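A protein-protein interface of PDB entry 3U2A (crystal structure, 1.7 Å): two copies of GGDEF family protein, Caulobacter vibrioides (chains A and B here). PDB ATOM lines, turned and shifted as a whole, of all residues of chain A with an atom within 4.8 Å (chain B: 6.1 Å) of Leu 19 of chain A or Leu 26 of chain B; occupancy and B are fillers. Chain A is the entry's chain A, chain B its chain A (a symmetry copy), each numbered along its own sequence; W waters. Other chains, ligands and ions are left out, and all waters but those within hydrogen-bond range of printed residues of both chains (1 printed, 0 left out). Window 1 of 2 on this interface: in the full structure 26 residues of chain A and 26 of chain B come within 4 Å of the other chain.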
ATOM      1  N   TRP A  10      14.335 -13.205 -18.708  1.00  0.00           N
ATOM      2  CA  TRP A  10      15.380 -12.521 -17.943  1.00  0.00           C
ATOM      3  C   TRP A  10      14.735 -11.543 -16.958  1.00  0.00           C
ATOM      4  O   TRP A  10      13.802 -10.825 -17.324  1.00  0.00           O
ATOM      5  CB  TRP A  10      16.349 -11.786 -18.884  1.00  0.00           C
ATOM      6  CG  TRP A  10      17.638 -11.406 -18.215  1.00  0.00           C
ATOM      7  CD1 TRP A  10      17.844 -10.357 -17.366  1.00  0.00           C
ATOM      8  CD2 TRP A  10      18.902 -12.085 -18.329  1.00  0.00           C
ATOM      9  NE1 TRP A  10      19.160 -10.333 -16.948  1.00  0.00           N
ATOM     10  CE2 TRP A  10      19.827 -11.388 -17.513  1.00  0.00           C
ATOM     11  CE3 TRP A  10      19.340 -13.209 -19.041  1.00  0.00           C
ATOM     12  CZ2 TRP A  10      21.169 -11.781 -17.393  1.00  0.00           C
ATOM     13  CZ3 TRP A  10      20.666 -13.600 -18.922  1.00  0.00           C
ATOM     14  CH2 TRP A  10      21.569 -12.889 -18.100  1.00  0.00           C
ATOM     15  N   THR A  15      20.054 -10.612 -13.723  1.00  0.00           N
ATOM     16  CA  THR A  15      21.027  -9.534 -13.858  1.00  0.00           C
ATOM     17  C   THR A  15      22.040  -9.554 -12.713  1.00  0.00           C
ATOM     18  O   THR A  15      23.243  -9.552 -12.962  1.00  0.00           O
ATOM     19  CB  THR A  15      20.337  -8.177 -14.036  1.00  0.00           C
ATOM     20  OG1 THR A  15      19.739  -8.153 -15.333  1.00  0.00           O
ATOM     21  CG2 THR A  15      21.327  -7.027 -13.936  1.00  0.00           C
ATOM     22  N   LEU A  16      21.566  -9.621 -11.470  1.00  0.00           N
ATOM     23  CA  LEU A  16      22.484  -9.629 -10.331  1.00  0.00           C
ATOM     24  C   LEU A  16      23.383 -10.872 -10.287  1.00  0.00           C
ATOM     25  O   LEU A  16      24.557 -10.769  -9.932  1.00  0.00           O
ATOM     26  CB  LEU A  16      21.737  -9.416  -9.013  1.00  0.00           C
ATOM     27  CG  LEU A  16      21.056  -8.054  -8.828  1.00  0.00           C
ATOM     28  CD1 LEU A  16      20.327  -8.012  -7.469  1.00  0.00           C
ATOM     29  CD2 LEU A  16      22.043  -6.863  -8.976  1.00  0.00           C
ATOM     30  N   GLU A  17      22.837 -12.026 -10.670  1.00  0.00           N
ATOM     31  CA  GLU A  17      23.593 -13.278 -10.726  1.00  0.00           C
ATOM     32  C   GLU A  17      24.759 -13.198 -11.702  1.00  0.00           C
ATOM     33  O   GLU A  17      25.876 -13.582 -11.356  1.00  0.00           O
ATOM     34  CB  GLU A  17      22.692 -14.458 -11.119  1.00  0.00           C
ATOM     35  CG  GLU A  17      21.779 -14.944 -10.018  1.00  0.00           C
ATOM     36  CD  GLU A  17      20.967 -16.157 -10.435  1.00  0.00           C
ATOM     37  OE1 GLU A  17      20.732 -16.341 -11.651  1.00  0.00           O
ATOM     38  OE2 GLU A  17      20.559 -16.924  -9.540  1.00  0.00           O
ATOM     39  N   ALA A  18      24.486 -12.715 -12.916  1.00  0.00           N
ATOM     40  CA  ALA A  18      25.515 -12.579 -13.945  1.00  0.00           C
ATOM     41  C   ALA A  18      26.573 -11.527 -13.575  1.00  0.00           C
ATOM     42  O   ALA A  18      27.763 -11.765 -13.741  1.00  0.00           O
ATOM     43  CB  ALA A  18      24.882 -12.270 -15.297  1.00  0.00           C
ATOM     44  N   LEU A  19      26.127 -10.372 -13.074  1.00  0.00           N
ATOM     45  CA  LEU A  19      27.029  -9.313 -12.606  1.00  0.00           C
ATOM     46  C   LEU A  19      27.932  -9.807 -11.469  1.00  0.00           C
ATOM     47  O   LEU A  19      29.153  -9.589 -11.482  1.00  0.00           O
ATOM     48  CB  LEU A  19      26.239  -8.064 -12.181  1.00  0.00           C
ATOM     49  CG  LEU A  19      25.523  -7.247 -13.273  1.00  0.00           C
ATOM     50  CD1 LEU A  19      24.659  -6.140 -12.660  1.00  0.00           C
ATOM     51  CD2 LEU A  19      26.521  -6.675 -14.275  1.00  0.00           C
ATOM     52  N   GLY A  20      27.331 -10.500 -10.509  1.00  0.00           N
ATOM     53  CA  GLY A  20      28.063 -11.067  -9.376  1.00  0.00           C
ATOM     54  C   GLY A  20      29.087 -12.096  -9.811  1.00  0.00           C
ATOM     55  O   GLY A  20      30.204 -12.128  -9.293  1.00  0.00           O
ATOM     56  N   ALA A  21      28.702 -12.936 -10.770  1.00  0.00           N
ATOM     57  CA  ALA A  21      29.556 -14.006 -11.280  1.00  0.00           C
ATOM     58  C   ALA A  21      30.778 -13.440 -12.001  1.00  0.00           C
ATOM     59  O   ALA A  21      31.887 -13.951 -11.860  1.00  0.00           O
ATOM     60  CB  ALA A  21      28.769 -14.907 -12.205  1.00  0.00           C
ATOM     61  N   ALA A  22      30.554 -12.369 -12.762  1.00  0.00           N
ATOM     62  CA  ALA A  22      31.609 -11.676 -13.487  1.00  0.00           C
ATOM     63  C   ALA A  22      32.446 -10.756 -12.589  1.00  0.00           C
ATOM     64  O   ALA A  22      33.548 -10.370 -12.967  1.00  0.00           O
ATOM     65  CB  ALA A  22      31.004 -10.895 -14.633  1.00  0.00           C
ATOM     66  N   ASP A  23      31.928 -10.434 -11.397  1.00  0.00           N
ATOM     67  CA  ASP A  23      32.544  -9.472 -10.466  1.00  0.00           C
ATOM     68  C   ASP A  23      32.573  -8.070 -11.073  1.00  0.00           C
ATOM     69  O   ASP A  23      33.585  -7.380 -11.024  1.00  0.00           O
ATOM     70  CB  ASP A  23      33.956  -9.906 -10.064  1.00  0.00           C
ATOM     71  CG  ASP A  23      34.420  -9.261  -8.773  1.00  0.00           C
ATOM     72  OD1 ASP A  23      33.551  -8.961  -7.926  1.00  0.00           O
ATOM     73  OD2 ASP A  23      35.650  -9.059  -8.606  1.00  0.00           O
ATOM     74  N   VAL A  24      31.444  -7.681 -11.658  1.00  0.00           N
ATOM     75  CA  VAL A  24      31.288  -6.428 -12.399  1.00  0.00           C
ATOM     76  C   VAL A  24      30.090  -5.647 -11.817  1.00  0.00           C
ATOM     77  O   VAL A  24      29.171  -6.256 -11.242  1.00  0.00           O
ATOM     78  CB  VAL A  24      31.078  -6.766 -13.921  1.00  0.00           C
ATOM     79  CG1 VAL A  24      30.309  -5.678 -14.692  1.00  0.00           C
ATOM     80  CG2 VAL A  24      32.411  -7.088 -14.590  1.00  0.00           C
ATOM     81  N   ALA A  25      30.076  -4.326 -11.988  1.00  0.00           N
ATOM     82  CA  ALA A  25      28.897  -3.534 -11.648  1.00  0.00           C
ATOM     83  C   ALA A  25      28.508  -2.626 -12.818  1.00  0.00           C
ATOM     84  O   ALA A  25      29.328  -2.326 -13.697  1.00  0.00           O
ATOM     85  CB  ALA A  25      29.111  -2.716 -10.371  1.00  0.00           C
ATOM     86  N   LEU A  26      27.246  -2.217 -12.843  1.00  0.00           N
ATOM     87  CA  LEU A  26      26.782  -1.261 -13.831  1.00  0.00           C
ATOM     88  C   LEU A  26      26.626   0.095 -13.151  1.00  0.00           C
ATOM     89  O   LEU A  26      26.336   0.165 -11.964  1.00  0.00           O
ATOM     90  CB  LEU A  26      25.455  -1.728 -14.422  1.00  0.00           C
ATOM     91  CG  LEU A  26      25.421  -3.137 -15.042  1.00  0.00           C
ATOM     92  CD1 LEU A  26      24.019  -3.492 -15.536  1.00  0.00           C
ATOM     93  CD2 LEU A  26      26.449  -3.257 -16.179  1.00  0.00           C
ATOM     94  N   ASN A  39      24.722  -0.809  -9.707  1.00  0.00           N
ATOM     95  CA  ASN A  39      24.003  -2.074  -9.630  1.00  0.00           C
ATOM     96  C   ASN A  39      24.960  -3.231  -9.919  1.00  0.00           C
ATOM     97  O   ASN A  39      25.687  -3.208 -10.909  1.00  0.00           O
ATOM     98  CB  ASN A  39      22.852  -2.087 -10.640  1.00  0.00           C
ATOM     99  CG  ASN A  39      21.921  -3.263 -10.449  1.00  0.00           C
ATOM    100  OD1 ASN A  39      21.677  -4.031 -11.380  1.00  0.00           O
ATOM    101  ND2 ASN A  39      21.379  -3.403  -9.239  1.00  0.00           N
ATOM    102  N   GLY A  40      24.950  -4.243  -9.061  1.00  0.00           N
ATOM    103  CA  GLY A  40      25.793  -5.421  -9.259  1.00  0.00           C
ATOM    104  C   GLY A  40      26.808  -5.569  -8.150  1.00  0.00           C
ATOM    105  O   GLY A  40      26.501  -5.309  -6.985  1.00  0.00           O
ATOM    106  N   ALA A  41      28.032  -5.950  -8.519  1.00  0.00           N
ATOM    107  CA  ALA A  41      29.060  -6.351  -7.548  1.00  0.00           C
ATOM    108  C   ALA A  41      29.814  -5.166  -6.935  1.00  0.00           C
ATOM    109  O   ALA A  41      31.052  -5.194  -6.815  1.00  0.00           O
ATOM    110  CB  ALA A  41      30.046  -7.371  -8.183  1.00  0.00           C
ATOM    111  N   THR B  15      19.487  -1.235 -16.558  1.00  0.00           N
ATOM    112  CA  THR B  15      20.378  -2.342 -16.891  1.00  0.00           C
ATOM    113  C   THR B  15      20.731  -2.343 -18.378  1.00  0.00           C
ATOM    114  O   THR B  15      21.908  -2.381 -18.725  1.00  0.00           O
ATOM    115  CB  THR B  15      19.814  -3.680 -16.398  1.00  0.00           C
ATOM    116  OG1 THR B  15      19.899  -3.695 -14.972  1.00  0.00           O
ATOM    117  CG2 THR B  15      20.606  -4.857 -16.945  1.00  0.00           C
ATOM    118  N   LEU B  19      24.527  -1.646 -19.993  1.00  0.00           N
ATOM    119  CA  LEU B  19      25.070  -2.727 -20.824  1.00  0.00           C
ATOM    120  C   LEU B  19      25.344  -2.252 -22.257  1.00  0.00           C
ATOM    121  O   LEU B  19      26.419  -2.505 -22.819  1.00  0.00           O
ATOM    122  CB  LEU B  19      24.137  -3.950 -20.817  1.00  0.00           C
ATOM    123  CG  LEU B  19      23.997  -4.754 -19.511  1.00  0.00           C
ATOM    124  CD1 LEU B  19      22.914  -5.831 -19.635  1.00  0.00           C
ATOM    125  CD2 LEU B  19      25.333  -5.362 -19.094  1.00  0.00           C
ATOM    126  N   VAL B  24      28.466  -4.480 -23.731  1.00  0.00           N
ATOM    127  CA  VAL B  24      28.641  -5.734 -22.995  1.00  0.00           C
ATOM    128  C   VAL B  24      27.288  -6.475 -22.938  1.00  0.00           C
ATOM    129  O   VAL B  24      26.225  -5.835 -23.015  1.00  0.00           O
ATOM    130  CB  VAL B  24      29.185  -5.400 -21.556  1.00  0.00           C
ATOM    131  CG1 VAL B  24      28.839  -6.471 -20.506  1.00  0.00           C
ATOM    132  CG2 VAL B  24      30.684  -5.122 -21.598  1.00  0.00           C
ATOM    133  N   ALA B  25      27.318  -7.796 -22.770  1.00  0.00           N
ATOM    134  CA  ALA B  25      26.096  -8.551 -22.507  1.00  0.00           C
ATOM    135  C   ALA B  25      26.279  -9.456 -21.286  1.00  0.00           C
ATOM    136  O   ALA B  25      27.408  -9.786 -20.896  1.00  0.00           O
ATOM    137  CB  ALA B  25      25.659  -9.366 -23.729  1.00  0.00           C
ATOM    138  N   LEU B  26      25.167  -9.828 -20.666  1.00  0.00           N
ATOM    139  CA  LEU B  26      25.196 -10.778 -19.569  1.00  0.00           C
ATOM    140  C   LEU B  26      24.699 -12.124 -20.085  1.00  0.00           C
ATOM    141  O   LEU B  26      23.881 -12.177 -20.995  1.00  0.00           O
ATOM    142  CB  LEU B  26      24.320 -10.276 -18.425  1.00  0.00           C
ATOM    143  CG  LEU B  26      24.623  -8.872 -17.873  1.00  0.00           C
ATOM    144  CD1 LEU B  26      23.630  -8.479 -16.778  1.00  0.00           C
ATOM    145  CD2 LEU B  26      26.069  -8.789 -17.356  1.00  0.00           C
ATOM    146  N   TRP B  27      25.203 -13.204 -19.507  1.00  0.00           N
ATOM    147  CA  TRP B  27      24.804 -14.547 -19.920  1.00  0.00           C
ATOM    148  C   TRP B  27      24.605 -15.445 -18.710  1.00  0.00           C
ATOM    149  O   TRP B  27      25.264 -15.273 -17.661  1.00  0.00           O
ATOM    150  CB  TRP B  27      25.820 -15.165 -20.902  1.00  0.00           C
ATOM    151  CG  TRP B  27      27.244 -15.275 -20.361  1.00  0.00           C
ATOM    152  CD1 TRP B  27      28.227 -14.337 -20.452  1.00  0.00           C
ATOM    153  CD2 TRP B  27      27.817 -16.392 -19.664  1.00  0.00           C
ATOM    154  NE1 TRP B  27      29.380 -14.794 -19.845  1.00  0.00           N
ATOM    155  CE2 TRP B  27      29.162 -16.055 -19.364  1.00  0.00           C
ATOM    156  CE3 TRP B  27      27.331 -17.647 -19.268  1.00  0.00           C
ATOM    157  CZ2 TRP B  27      30.024 -16.924 -18.676  1.00  0.00           C
ATOM    158  CZ3 TRP B  27      28.191 -18.518 -18.586  1.00  0.00           C
ATOM    159  CH2 TRP B  27      29.521 -18.150 -18.291  1.00  0.00           C
ATOM    160  N   ILE B  28      23.661 -16.376 -18.859  1.00  0.00           N
ATOM    161  CA  ILE B  28      23.474 -17.482 -17.929  1.00  0.00           C
ATOM    162  C   ILE B  28      23.389 -18.770 -18.744  1.00  0.00           C
ATOM    163  O   ILE B  28      22.655 -18.835 -19.731  1.00  0.00           O
ATOM    164  CB  ILE B  28      22.212 -17.307 -17.048  1.00  0.00           C
ATOM    165  CG1 ILE B  28      22.361 -16.078 -16.139  1.00  0.00           C
ATOM    166  CG2 ILE B  28      21.975 -18.556 -16.186  1.00  0.00           C
ATOM    167  CD1 ILE B  28      21.095 -15.662 -15.430  1.00  0.00           C
ATOM    168  N   ARG B  37      21.088 -18.084 -21.920  1.00  0.00           N
ATOM    169  CA  ARG B  37      20.351 -16.822 -21.993  1.00  0.00           C
ATOM    170  C   ARG B  37      21.285 -15.626 -22.088  1.00  0.00           C
ATOM    171  O   ARG B  37      22.326 -15.591 -21.425  1.00  0.00           O
ATOM    172  CB  ARG B  37      19.424 -16.680 -20.777  1.00  0.00           C
ATOM    173  CG  ARG B  37      18.249 -17.664 -20.779  1.00  0.00           C
ATOM    174  CD  ARG B  37      17.920 -18.144 -19.365  1.00  0.00           C
ATOM    175  NE  ARG B  37      17.411 -17.086 -18.519  1.00  0.00           N
ATOM    176  CZ  ARG B  37      17.544 -17.034 -17.195  1.00  0.00           C
ATOM    177  NH1 ARG B  37      18.204 -17.978 -16.520  1.00  0.00           N
ATOM    178  NH2 ARG B  37      17.031 -16.014 -16.539  1.00  0.00           N
ATOM    179  N   LEU B  38      20.901 -14.649 -22.916  1.00  0.00           N
ATOM    180  CA  LEU B  38      21.649 -13.400 -23.076  1.00  0.00           C
ATOM    181  C   LEU B  38      20.794 -12.162 -22.809  1.00  0.00           C
ATOM    182  O   LEU B  38      19.596 -12.142 -23.119  1.00  0.00           O
ATOM    183  CB  LEU B  38      22.239 -13.310 -24.484  1.00  0.00           C
ATOM    184  CG  LEU B  38      23.400 -14.242 -24.797  1.00  0.00           C
ATOM    185  CD1 LEU B  38      23.513 -14.424 -26.310  1.00  0.00           C
ATOM    186  CD2 LEU B  38      24.698 -13.685 -24.220  1.00  0.00           C
ATOM    187  N   ASN B  39      21.422 -11.140 -22.229  1.00  0.00           N
ATOM    188  CA  ASN B  39      20.789  -9.854 -21.968  1.00  0.00           C
ATOM    189  C   ASN B  39      21.802  -8.727 -22.172  1.00  0.00           C
ATOM    190  O   ASN B  39      22.909  -8.778 -21.643  1.00  0.00           O
ATOM    191  CB  ASN B  39      20.252  -9.815 -20.534  1.00  0.00           C
ATOM    192  CG  ASN B  39      19.375  -8.611 -20.272  1.00  0.00           C
ATOM    193  OD1 ASN B  39      19.622  -7.843 -19.341  1.00  0.00           O
ATOM    194  ND2 ASN B  39      18.331  -8.446 -21.084  1.00  0.00           N
ATOM    195  N   GLY B  40      21.417  -7.709 -22.932  1.00  0.00           N
ATOM    196  CA  GLY B  40      22.289  -6.557 -23.163  1.00  0.00           C
ATOM    197  C   GLY B  40      22.664  -6.431 -24.621  1.00  0.00           C
ATOM    198  O   GLY B  40      21.836  -6.674 -25.502  1.00  0.00           O
ATOM    199  N   ALA B  41      23.927  -6.089 -24.876  1.00  0.00           N
ATOM    200  CA  ALA B  41      24.387  -5.710 -26.220  1.00  0.00           C
ATOM    201  C   ALA B  41      24.728  -6.913 -27.108  1.00  0.00           C
ATOM    202  O   ALA B  41      25.764  -6.919 -27.798  1.00  0.00           O
ATOM    203  CB  ALA B  41      25.585  -4.724 -26.133  1.00  0.00           C
ATOM    204  N   GLY B 111      27.817 -14.881 -16.275  1.00  0.00           N
ATOM    205  CA  GLY B 111      28.886 -13.915 -16.371  1.00  0.00           C
ATOM    206  C   GLY B 111      28.632 -12.832 -17.386  1.00  0.00           C
ATOM    207  O   GLY B 111      27.477 -12.531 -17.724  1.00  0.00           O
ATOM    208  N   VAL B 112      29.736 -12.249 -17.845  1.00  0.00           N
ATOM    209  CA  VAL B 112      29.715 -11.167 -18.830  1.00  0.00           C
ATOM    210  C   VAL B 112      30.392 -11.596 -20.129  1.00  0.00           C
ATOM    211  O   VAL B 112      31.263 -12.485 -20.139  1.00  0.00           O
ATOM    212  CB  VAL B 112      30.386  -9.872 -18.264  1.00  0.00           C
ATOM    213  CG1 VAL B 112      30.610  -8.820 -19.354  1.00  0.00           C
ATOM    214  CG2 VAL B 112      29.525  -9.281 -17.169  1.00  0.00           C
ATOM    215  N   VAL B 113      29.980 -10.982 -21.227  1.00  0.00           N
ATOM    216  CA  VAL B 113      30.684 -11.133 -22.485  1.00  0.00           C
ATOM    217  C   VAL B 113      30.952  -9.729 -23.018  1.00  0.00           C
ATOM    218  O   VAL B 113      30.078  -8.842 -22.981  1.00  0.00           O
ATOM    219  CB  VAL B 113      29.953 -12.065 -23.494  1.00  0.00           C
ATOM    220  CG1 VAL B 113      28.505 -11.643 -23.694  1.00  0.00           C
ATOM    221  CG2 VAL B 113      30.686 -12.103 -24.815  1.00  0.00           C
HETATM  222  O   HOH W   1      18.371 -16.897 -13.284  1.00  0.00           O
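NE1 of Trp 10 of chain A is in hydrogen-bond range of OD1 of Asn 39 of chain B.
The indole nitrogen of Trp 10 of chain A lies within hydrogen-bond range of the side-chain hydroxyl of Thr 15 of chain A. The backbone carbonyl oxygen (O) of Leu 19 of chain A sits at hydrogen-bond distance from the backbone NH (N) of Val 24 of chain A (3.0 Å). The backbone NH of Leu 26 of chain A sits at hydrogen-bond distance from the backbone carbonyl oxygen of Asn 39 of chain A (2.7 Å). The backbone NH of Val 24 of chain B lies within hydrogen-bond range of the backbone carbonyl oxygen of Leu 19 of chain B (3.0 Å). The backbone carbonyl oxygen (O) of Asn 39 of chain B lies within hydrogen-bond range of the backbone NH (N) of Leu 26 of chain B. The indole nitrogen (NE1) of Trp 27 of chain B sits at hydrogen-bond distance from the backbone carbonyl oxygen (O) of Val 112 of chain B.
Among the printed residues, pairs that only touch across the chains: Trp 10 of chain A with Leu 26 of chain B, Trp 10 of chain A with Trp 27 of chain B, Trp 10 of chain A with Ile 28 of chain B, Trp 10 of chain A with Arg 37 of chain B, Thr 15 of chain A with Thr 15 of chain B, Thr 15 of chain A with Leu 26 of chain B, Glu 17 of chain A with Ile 28 of chain B, Ala 18 of chain A with Leu 26 of chain B, Ala 18 of chain A with Trp 27 of chain B, Ala 18 of chain A with Gly 111 of chain B, Leu 19 of chain A with Leu 26 of chain B, Ala 22 of chain A with Val 112 of chain B, Leu 26 of chain A with Thr 15 of chain B and Leu 26 of chain A with Leu 19 of chain B.
Leu 19 of chain A touches just one residue of chain B: Leu 26 (3.8 Å). Of chain A, only Trp 10 (3.6 Å), Thr 15 (3.9 Å), Ala 18 (3.8 Å) and Leu 19 (3.8 Å) come within 4 Å of Leu 26 of chain B. Printed residues of chain B within 4 Å of Thr 15 of chain A: Thr 15 (3.8 Å) and Leu 26 (3.9 Å). Of the printed residues of chain A, Ile 28 of chain B touches Trp 10 (3.8 Å) and Glu 17 (3.9 Å). The nearest printed residue of chain A that does not touch Leu 26 of chain B is Leu 26 of chain A (5.2 Å). The nearest printed residue of chain A that does not touch Thr 15 of chain B is Asn 39 of chain A (4.02 Å).
Printed residues of chain A that touch a printed residue of chain B: Trp 10, Thr 15, Glu 17, Ala 18, Leu 19, Ala 22 and Leu 26. Of the 15 printed residues of chain B, 9 touch a printed residue of chain A.
Thr 15 of chain A touches its own counterpart, Thr 15 of chain B. Thr 15 of chain A touches Leu 26 of chain B, and with the chains exchanged Leu 26 of chain A touches Thr 15 of chain B. Leu 19 of chain A touches Leu 26 of chain B, and with the chains exchanged Leu 26 of chain A touches Leu 19 of chain B. Positions printed for both chains: 15, 19, 24, 25, 26, 39, 40 and 41. Of the 15 pairs that touch across the chains among the printed residues, 5 have their exchanged pair printed and touching as well.
Water W1 bridges OE1 of Glu 17 of chain A (2.9 Å) and NH1 of Arg 37 of chain B (3.4 Å).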
